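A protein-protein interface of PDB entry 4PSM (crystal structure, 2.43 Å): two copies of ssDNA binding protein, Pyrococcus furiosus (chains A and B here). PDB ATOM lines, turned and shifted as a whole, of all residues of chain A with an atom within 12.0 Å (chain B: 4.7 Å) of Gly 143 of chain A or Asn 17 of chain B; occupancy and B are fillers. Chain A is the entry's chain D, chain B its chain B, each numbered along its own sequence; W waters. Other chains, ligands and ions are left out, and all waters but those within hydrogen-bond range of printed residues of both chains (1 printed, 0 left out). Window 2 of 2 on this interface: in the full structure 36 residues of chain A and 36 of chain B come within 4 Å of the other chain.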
ATOM      1  N   VAL A 134      24.883 -24.248   0.728  1.00  0.00           N
ATOM      2  CA  VAL A 134      24.035 -23.069   0.620  1.00  0.00           C
ATOM      3  C   VAL A 134      22.565 -23.405   0.875  1.00  0.00           C
ATOM      4  O   VAL A 134      21.896 -22.724   1.660  1.00  0.00           O
ATOM      5  CB  VAL A 134      24.195 -22.395  -0.754  1.00  0.00           C
ATOM      6  CG1 VAL A 134      23.114 -21.350  -0.973  1.00  0.00           C
ATOM      7  CG2 VAL A 134      25.580 -21.777  -0.866  1.00  0.00           C
ATOM      8  N   GLU A 135      22.069 -24.457   0.223  1.00  0.00           N
ATOM      9  CA  GLU A 135      20.685 -24.866   0.404  1.00  0.00           C
ATOM     10  C   GLU A 135      20.428 -25.259   1.851  1.00  0.00           C
ATOM     11  O   GLU A 135      19.366 -24.987   2.395  1.00  0.00           O
ATOM     12  CB  GLU A 135      20.319 -26.023  -0.524  1.00  0.00           C
ATOM     13  CG  GLU A 135      18.841 -26.424  -0.423  1.00  0.00           C
ATOM     14  CD  GLU A 135      17.878 -25.352  -0.945  1.00  0.00           C
ATOM     15  OE1 GLU A 135      18.345 -24.333  -1.499  1.00  0.00           O
ATOM     16  OE2 GLU A 135      16.645 -25.532  -0.802  1.00  0.00           O
ATOM     17  N   ARG A 136      21.422 -25.890   2.465  1.00  0.00           N
ATOM     18  CA  ARG A 136      21.332 -26.319   3.852  1.00  0.00           C
ATOM     19  C   ARG A 136      21.204 -25.110   4.794  1.00  0.00           C
ATOM     20  O   ARG A 136      20.437 -25.137   5.761  1.00  0.00           O
ATOM     21  CB  ARG A 136      22.557 -27.167   4.206  1.00  0.00           C
ATOM     22  CG  ARG A 136      22.300 -28.257   5.230  1.00  0.00           C
ATOM     23  CD  ARG A 136      23.505 -29.177   5.371  1.00  0.00           C
ATOM     24  NE  ARG A 136      23.941 -29.702   4.113  1.00  0.00           N
ATOM     25  CZ  ARG A 136      25.139 -29.724   3.536  1.00  0.00           C
ATOM     26  NH1 ARG A 136      25.165 -30.298   2.350  1.00  0.00           N
ATOM     27  NH2 ARG A 136      26.263 -29.236   4.055  1.00  0.00           N
ATOM     28  N   MET A 137      21.951 -24.050   4.501  1.00  0.00           N
ATOM     29  CA  MET A 137      21.852 -22.818   5.269  1.00  0.00           C
ATOM     30  C   MET A 137      20.485 -22.178   5.110  1.00  0.00           C
ATOM     31  O   MET A 137      19.967 -21.590   6.049  1.00  0.00           O
ATOM     32  CB  MET A 137      22.917 -21.820   4.835  1.00  0.00           C
ATOM     33  CG  MET A 137      24.314 -22.162   5.290  1.00  0.00           C
ATOM     34  SD  MET A 137      25.634 -21.059   4.383  1.00  0.00           S
ATOM     35  CE  MET A 137      24.789 -19.313   4.634  1.00  0.00           C
ATOM     36  N   LYS A 138      19.916 -22.277   3.912  1.00  0.00           N
ATOM     37  CA  LYS A 138      18.583 -21.765   3.683  1.00  0.00           C
ATOM     38  C   LYS A 138      17.627 -22.506   4.609  1.00  0.00           C
ATOM     39  O   LYS A 138      16.778 -21.900   5.259  1.00  0.00           O
ATOM     40  CB  LYS A 138      18.164 -21.947   2.231  1.00  0.00           C
ATOM     41  CG  LYS A 138      18.775 -20.936   1.280  1.00  0.00           C
ATOM     42  CD  LYS A 138      18.457 -21.283  -0.169  1.00  0.00           C
ATOM     43  CE  LYS A 138      16.975 -21.127  -0.490  1.00  0.00           C
ATOM     44  NZ  LYS A 138      16.630 -21.736  -1.813  1.00  0.00           N
ATOM     45  N   GLN A 139      17.803 -23.820   4.684  1.00  0.00           N
ATOM     46  CA  GLN A 139      16.957 -24.685   5.494  1.00  0.00           C
ATOM     47  C   GLN A 139      17.075 -24.420   6.990  1.00  0.00           C
ATOM     48  O   GLN A 139      16.085 -24.468   7.732  1.00  0.00           O
ATOM     49  CB  GLN A 139      17.330 -26.143   5.239  1.00  0.00           C
ATOM     50  CG  GLN A 139      17.109 -26.604   3.830  1.00  0.00           C
ATOM     51  CD  GLN A 139      17.705 -27.973   3.585  1.00  0.00           C
ATOM     52  OE1 GLN A 139      18.533 -28.460   4.364  1.00  0.00           O
ATOM     53  NE2 GLN A 139      17.289 -28.603   2.495  1.00  0.00           N
ATOM     54  N   GLU A 140      18.299 -24.158   7.432  1.00  0.00           N
ATOM     55  CA  GLU A 140      18.585 -24.131   8.856  1.00  0.00           C
ATOM     56  C   GLU A 140      18.627 -22.741   9.486  1.00  0.00           C
ATOM     57  O   GLU A 140      18.476 -22.612  10.696  1.00  0.00           O
ATOM     58  CB  GLU A 140      19.885 -24.881   9.129  1.00  0.00           C
ATOM     59  CG  GLU A 140      19.823 -26.357   8.750  1.00  0.00           C
ATOM     60  CD  GLU A 140      21.026 -27.147   9.245  1.00  0.00           C
ATOM     61  OE1 GLU A 140      21.967 -26.526   9.787  1.00  0.00           O
ATOM     62  OE2 GLU A 140      21.030 -28.389   9.093  1.00  0.00           O
ATOM     63  N   TYR A 141      18.811 -21.706   8.673  1.00  0.00           N
ATOM     64  CA  TYR A 141      19.070 -20.372   9.204  1.00  0.00           C
ATOM     65  C   TYR A 141      18.205 -19.294   8.569  1.00  0.00           C
ATOM     66  O   TYR A 141      18.434 -18.105   8.785  1.00  0.00           O
ATOM     67  CB  TYR A 141      20.552 -19.997   9.030  1.00  0.00           C
ATOM     68  CG  TYR A 141      21.525 -20.963   9.667  1.00  0.00           C
ATOM     69  CD1 TYR A 141      21.598 -21.104  11.046  1.00  0.00           C
ATOM     70  CD2 TYR A 141      22.378 -21.726   8.891  1.00  0.00           C
ATOM     71  CE1 TYR A 141      22.489 -21.990  11.628  1.00  0.00           C
ATOM     72  CE2 TYR A 141      23.267 -22.610   9.461  1.00  0.00           C
ATOM     73  CZ  TYR A 141      23.322 -22.739  10.825  1.00  0.00           C
ATOM     74  OH  TYR A 141      24.217 -23.625  11.371  1.00  0.00           O
ATOM     75  N   THR A 142      17.224 -19.693   7.770  1.00  0.00           N
ATOM     76  CA  THR A 142      16.394 -18.707   7.081  1.00  0.00           C
ATOM     77  C   THR A 142      14.963 -19.194   6.874  1.00  0.00           C
ATOM     78  O   THR A 142      14.666 -20.379   7.042  1.00  0.00           O
ATOM     79  CB  THR A 142      16.976 -18.309   5.684  1.00  0.00           C
ATOM     80  OG1 THR A 142      16.570 -19.262   4.695  1.00  0.00           O
ATOM     81  CG2 THR A 142      18.503 -18.211   5.707  1.00  0.00           C
ATOM     82  N   GLY A 143      14.086 -18.268   6.497  1.00  0.00           N
ATOM     83  CA  GLY A 143      12.750 -18.606   6.045  1.00  0.00           C
ATOM     84  C   GLY A 143      12.631 -18.565   4.526  1.00  0.00           C
ATOM     85  O   GLY A 143      11.525 -18.525   3.996  1.00  0.00           O
ATOM     86  N   LEU A 144      13.763 -18.580   3.817  1.00  0.00           N
ATOM     87  CA  LEU A 144      13.739 -18.466   2.351  1.00  0.00           C
ATOM     88  C   LEU A 144      13.040 -19.635   1.660  1.00  0.00           C
ATOM     89  O   LEU A 144      13.078 -20.766   2.139  1.00  0.00           O
ATOM     90  CB  LEU A 144      15.151 -18.285   1.779  1.00  0.00           C
ATOM     91  CG  LEU A 144      15.773 -16.949   2.204  1.00  0.00           C
ATOM     92  CD1 LEU A 144      17.259 -16.791   1.935  1.00  0.00           C
ATOM     93  CD2 LEU A 144      14.946 -15.701   1.843  1.00  0.00           C
ATOM     94  N   LYS A 145      12.389 -19.353   0.538  1.00  0.00           N
ATOM     95  CA  LYS A 145      11.788 -20.409  -0.265  1.00  0.00           C
ATOM     96  C   LYS A 145      12.844 -21.467  -0.565  1.00  0.00           C
ATOM     97  O   LYS A 145      13.948 -21.143  -1.007  1.00  0.00           O
ATOM     98  CB  LYS A 145      11.231 -19.834  -1.568  1.00  0.00           C
ATOM     99  CG  LYS A 145      10.373 -20.803  -2.366  1.00  0.00           C
ATOM    100  CD  LYS A 145       9.731 -20.123  -3.574  1.00  0.00           C
ATOM    101  CE  LYS A 145       8.813 -18.965  -3.170  1.00  0.00           C
ATOM    102  NZ  LYS A 145       9.553 -17.734  -2.749  1.00  0.00           N
ATOM    103  N   LEU A 146      12.513 -22.728  -0.302  1.00  0.00           N
ATOM    104  CA  LEU A 146      13.458 -23.818  -0.532  1.00  0.00           C
ATOM    105  C   LEU A 146      13.219 -24.503  -1.875  1.00  0.00           C
ATOM    106  O   LEU A 146      12.108 -24.471  -2.418  1.00  0.00           O
ATOM    107  CB  LEU A 146      13.391 -24.855   0.595  1.00  0.00           C
ATOM    108  CG  LEU A 146      13.568 -24.351   2.032  1.00  0.00           C
ATOM    109  CD1 LEU A 146      13.406 -25.453   3.078  1.00  0.00           C
ATOM    110  CD2 LEU A 146      14.847 -23.542   2.250  1.00  0.00           C
ATOM    111  N   ARG A 147      14.268 -25.126  -2.402  1.00  0.00           N
ATOM    112  CA  ARG A 147      14.154 -25.917  -3.627  1.00  0.00           C
ATOM    113  C   ARG A 147      13.193 -27.088  -3.428  1.00  0.00           C
ATOM    114  O   ARG A 147      12.505 -27.511  -4.359  1.00  0.00           O
ATOM    115  CB  ARG A 147      15.529 -26.443  -4.056  1.00  0.00           C
ATOM    116  CG  ARG A 147      16.552 -25.357  -4.345  1.00  0.00           C
ATOM    117  CD  ARG A 147      16.153 -24.530  -5.556  1.00  0.00           C
ATOM    118  NE  ARG A 147      16.915 -23.289  -5.642  1.00  0.00           N
ATOM    119  CZ  ARG A 147      18.126 -23.190  -6.182  1.00  0.00           C
ATOM    120  NH1 ARG A 147      18.718 -24.267  -6.686  1.00  0.00           N
ATOM    121  NH2 ARG A 147      18.746 -22.015  -6.215  1.00  0.00           N
ATOM    122  N   SER A 148      13.151 -27.603  -2.204  1.00  0.00           N
ATOM    123  CA  SER A 148      12.337 -28.769  -1.884  1.00  0.00           C
ATOM    124  C   SER A 148      10.879 -28.395  -1.645  1.00  0.00           C
ATOM    125  O   SER A 148      10.082 -29.224  -1.207  1.00  0.00           O
ATOM    126  CB  SER A 148      12.906 -29.500  -0.664  1.00  0.00           C
ATOM    127  OG  SER A 148      12.820 -28.691   0.504  1.00  0.00           O
ATOM    128  N   GLU A 149      10.543 -27.142  -1.934  1.00  0.00           N
ATOM    129  CA  GLU A 149       9.174 -26.661  -1.793  1.00  0.00           C
ATOM    130  C   GLU A 149       8.499 -26.534  -3.149  1.00  0.00           C
ATOM    131  O   GLU A 149       8.569 -25.487  -3.787  1.00  0.00           O
ATOM    132  CB  GLU A 149       9.145 -25.311  -1.075  1.00  0.00           C
ATOM    133  CG  GLU A 149       9.390 -25.391   0.420  1.00  0.00           C
ATOM    134  CD  GLU A 149       9.213 -24.051   1.103  1.00  0.00           C
ATOM    135  OE1 GLU A 149       8.389 -23.967   2.039  1.00  0.00           O
ATOM    136  OE2 GLU A 149       9.898 -23.083   0.705  1.00  0.00           O
ATOM    137  N   GLY B  14       7.463 -15.433  13.881  1.00  0.00           N
ATOM    138  CA  GLY B  14       8.388 -16.292  13.173  1.00  0.00           C
ATOM    139  C   GLY B  14       8.533 -17.680  13.764  1.00  0.00           C
ATOM    140  O   GLY B  14       9.606 -18.276  13.685  1.00  0.00           O
ATOM    141  N   TYR B  15       7.457 -18.208  14.339  1.00  0.00           N
ATOM    142  CA  TYR B  15       7.510 -19.531  14.949  1.00  0.00           C
ATOM    143  C   TYR B  15       7.632 -20.601  13.861  1.00  0.00           C
ATOM    144  O   TYR B  15       8.406 -21.556  13.996  1.00  0.00           O
ATOM    145  CB  TYR B  15       6.264 -19.798  15.813  1.00  0.00           C
ATOM    146  CG  TYR B  15       5.085 -20.283  15.009  1.00  0.00           C
ATOM    147  CD1 TYR B  15       4.937 -21.638  14.698  1.00  0.00           C
ATOM    148  CD2 TYR B  15       4.138 -19.390  14.528  1.00  0.00           C
ATOM    149  CE1 TYR B  15       3.868 -22.090  13.937  1.00  0.00           C
ATOM    150  CE2 TYR B  15       3.062 -19.830  13.766  1.00  0.00           C
ATOM    151  CZ  TYR B  15       2.930 -21.182  13.481  1.00  0.00           C
ATOM    152  OH  TYR B  15       1.863 -21.624  12.736  1.00  0.00           O
ATOM    153  N   ALA B  16       6.870 -20.436  12.783  1.00  0.00           N
ATOM    154  CA  ALA B  16       6.791 -21.481  11.762  1.00  0.00           C
ATOM    155  C   ALA B  16       8.129 -21.711  11.059  1.00  0.00           C
ATOM    156  O   ALA B  16       8.534 -22.859  10.851  1.00  0.00           O
ATOM    157  CB  ALA B  16       5.670 -21.196  10.758  1.00  0.00           C
ATOM    158  N   ASN B  17       8.823 -20.630  10.713  1.00  0.00           N
ATOM    159  CA  ASN B  17      10.167 -20.768  10.137  1.00  0.00           C
ATOM    160  C   ASN B  17      11.137 -21.441  11.109  1.00  0.00           C
ATOM    161  O   ASN B  17      11.992 -22.238  10.706  1.00  0.00           O
ATOM    162  CB  ASN B  17      10.728 -19.412   9.688  1.00  0.00           C
ATOM    163  CG  ASN B  17      10.117 -18.918   8.381  1.00  0.00           C
ATOM    164  OD1 ASN B  17       9.704 -19.710   7.532  1.00  0.00           O
ATOM    165  ND2 ASN B  17      10.067 -17.600   8.214  1.00  0.00           N
ATOM    166  N   LYS B  18      10.995 -21.123  12.393  1.00  0.00           N
ATOM    167  CA  LYS B  18      11.916 -21.642  13.393  1.00  0.00           C
ATOM    168  C   LYS B  18      11.716 -23.134  13.573  1.00  0.00           C
ATOM    169  O   LYS B  18      12.687 -23.883  13.696  1.00  0.00           O
ATOM    170  CB  LYS B  18      11.742 -20.922  14.737  1.00  0.00           C
ATOM    171  CG  LYS B  18      12.780 -21.327  15.782  1.00  0.00           C
ATOM    172  CD  LYS B  18      14.202 -21.019  15.299  1.00  0.00           C
ATOM    173  CE  LYS B  18      15.233 -21.198  16.412  1.00  0.00           C
ATOM    174  NZ  LYS B  18      14.967 -20.278  17.573  1.00  0.00           N
ATOM    175  N   VAL B  19      10.452 -23.557  13.597  1.00  0.00           N
ATOM    176  CA  VAL B  19      10.127 -24.971  13.676  1.00  0.00           C
ATOM    177  C   VAL B  19      10.806 -25.724  12.535  1.00  0.00           C
ATOM    178  O   VAL B  19      11.504 -26.715  12.760  1.00  0.00           O
ATOM    179  CB  VAL B  19       8.605 -25.199  13.623  1.00  0.00           C
ATOM    180  CG1 VAL B  19       8.286 -26.668  13.387  1.00  0.00           C
ATOM    181  CG2 VAL B  19       7.948 -24.706  14.907  1.00  0.00           C
ATOM    182  N   ARG B  20      10.613 -25.236  11.313  1.00  0.00           N
ATOM    183  CA  ARG B  20      11.160 -25.895  10.136  1.00  0.00           C
ATOM    184  C   ARG B  20      12.683 -25.953  10.205  1.00  0.00           C
ATOM    185  O   ARG B  20      13.287 -26.967   9.873  1.00  0.00           O
ATOM    186  CB  ARG B  20      10.711 -25.181   8.859  1.00  0.00           C
ATOM    187  CG  ARG B  20      10.820 -26.046   7.614  1.00  0.00           C
ATOM    188  CD  ARG B  20      10.445 -25.261   6.372  1.00  0.00           C
ATOM    189  NE  ARG B  20      11.455 -24.251   6.066  1.00  0.00           N
ATOM    190  CZ  ARG B  20      11.403 -23.430   5.022  1.00  0.00           C
ATOM    191  NH1 ARG B  20      10.384 -23.494   4.173  1.00  0.00           N
ATOM    192  NH2 ARG B  20      12.371 -22.541   4.832  1.00  0.00           N
ATOM    193  N   ARG B  21      13.297 -24.868  10.667  1.00  0.00           N
ATOM    194  CA  ARG B  21      14.750 -24.809  10.742  1.00  0.00           C
ATOM    195  C   ARG B  21      15.316 -25.842  11.701  1.00  0.00           C
ATOM    196  O   ARG B  21      16.272 -26.554  11.384  1.00  0.00           O
ATOM    197  CB  ARG B  21      15.210 -23.409  11.114  1.00  0.00           C
ATOM    198  CG  ARG B  21      15.030 -22.418   9.986  1.00  0.00           C
ATOM    199  CD  ARG B  21      15.116 -20.995  10.484  1.00  0.00           C
ATOM    200  NE  ARG B  21      16.307 -20.788  11.289  1.00  0.00           N
ATOM    201  CZ  ARG B  21      16.586 -19.651  11.907  1.00  0.00           C
ATOM    202  NH1 ARG B  21      15.743 -18.634  11.799  1.00  0.00           N
ATOM    203  NH2 ARG B  21      17.698 -19.530  12.625  1.00  0.00           N
ATOM    204  N   GLU B 110      19.275 -13.068   5.604  1.00  0.00           N
ATOM    205  CA  GLU B 110      18.684 -13.745   4.464  1.00  0.00           C
ATOM    206  C   GLU B 110      19.060 -13.072   3.147  1.00  0.00           C
ATOM    207  O   GLU B 110      19.203 -13.729   2.109  1.00  0.00           O
ATOM    208  CB  GLU B 110      17.164 -13.816   4.619  1.00  0.00           C
ATOM    209  CG  GLU B 110      16.712 -14.812   5.678  1.00  0.00           C
ATOM    210  CD  GLU B 110      15.213 -14.945   5.745  1.00  0.00           C
ATOM    211  OE1 GLU B 110      14.526 -14.289   4.932  1.00  0.00           O
ATOM    212  OE2 GLU B 110      14.726 -15.703   6.611  1.00  0.00           O
HETATM  213  O   HOH W   1      13.716 -23.561   7.266  1.00  0.00           O
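Among the printed residues, pairs that only touch across the chains: Gln 139 of chain A with Arg 21 of chain B, Tyr 141 of chain A with Arg 21 of chain B, Thr 142 of chain A with Arg 20 of chain B, Thr 142 of chain A with Arg 21 of chain B, Thr 142 of chain A with Glu 110 of chain B, Gly 143 of chain A with Asn 17 of chain B, Gly 143 of chain A with Arg 20 of chain B, Leu 144 of chain A with Glu 110 of chain B and Leu 146 of chain A with Arg 20 of chain B.
Water W1 lies within hydrogen-bond range of O of Gln 139 of chain A, NE of Arg 20 of chain B and O of Thr 142 of chain A.
Printed residues of chain B within 4 Å of Thr 142 of chain A: Arg 20 (3.9 Å), Arg 21 (3.5 Å) and Glu 110 (3.5 Å). Of the printed residues of chain B, Gly 143 of chain A touches Asn 17, Arg 20 and Glu 110. Printed residues of chain B within 4 Å of Leu 146 of chain A: Arg 20. Arg 147 of chain A touches none of the printed residues of chain B. No residue of chain A comes within 4 Å of Ala 16 of chain B. Asn 17 of chain B touches just one residue of chain A: Gly 143. No residue of chain A comes within 4 Å of Lys 18 of chain B. No residue of chain A comes within 4 Å of Val 19 of chain B. Of the printed residues of chain A, Arg 21 of chain B touches Gln 139, Glu 140, Tyr 141 and Thr 142. The nearest printed residue of chain B that does not touch Gly 143 of chain A is Arg 21 of chain B (4.9 Å).
OG1 of Thr 142 of chain A is in hydrogen-bond range of O of Lys 138 of chain A, 2.7 Å away. The backbone NH (N) of Leu 144 of chain A sits at hydrogen-bond distance from the side-chain hydroxyl (OG1) of Thr 142 of chain A (3.0 Å). The backbone NH (N) of Leu 146 of chain A lies within hydrogen-bond range of the side-chain carboxylate (OE2) of Glu 149 of chain A, at 2.8 Å.
No position is printed for both chains. Of the 13 pairs that touch across the chains among the printed residues, none has its exchanged pair printed and touching as well.
The guanidinium group (NH2) of Arg 20 of chain B lies within hydrogen-bond range of the backbone carbonyl oxygen (O) of Leu 144 of chain A (3.3 Å). The side-chain carboxylate (OE1) of Glu 149 of chain A lies within salt-bridge range of the guanidinium group (NH1) of Arg 20 of chain B (3.0 Å). O of Glu 140 of chain A sits at hydrogen-bond distance from NE of Arg 21 of chain B (2.9 Å). OE2 of Glu 110 of chain B sits at hydrogen-bond distance from N of Gly 143 of chain A, at 2.6 Å.
Of the 9 printed residues of chain B, 4 touch a printed residue of chain A. Printed residues of chain B that touch a printed residue of chain A: Asn 17, Arg 20, Arg 21 and Glu 110. Hydrophobic or aromatic side chains of chain A within 4 Å of the printed part of chain B: Leu 144 and Leu 146. Among the printed residues, 13 pairs touch across the chains.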
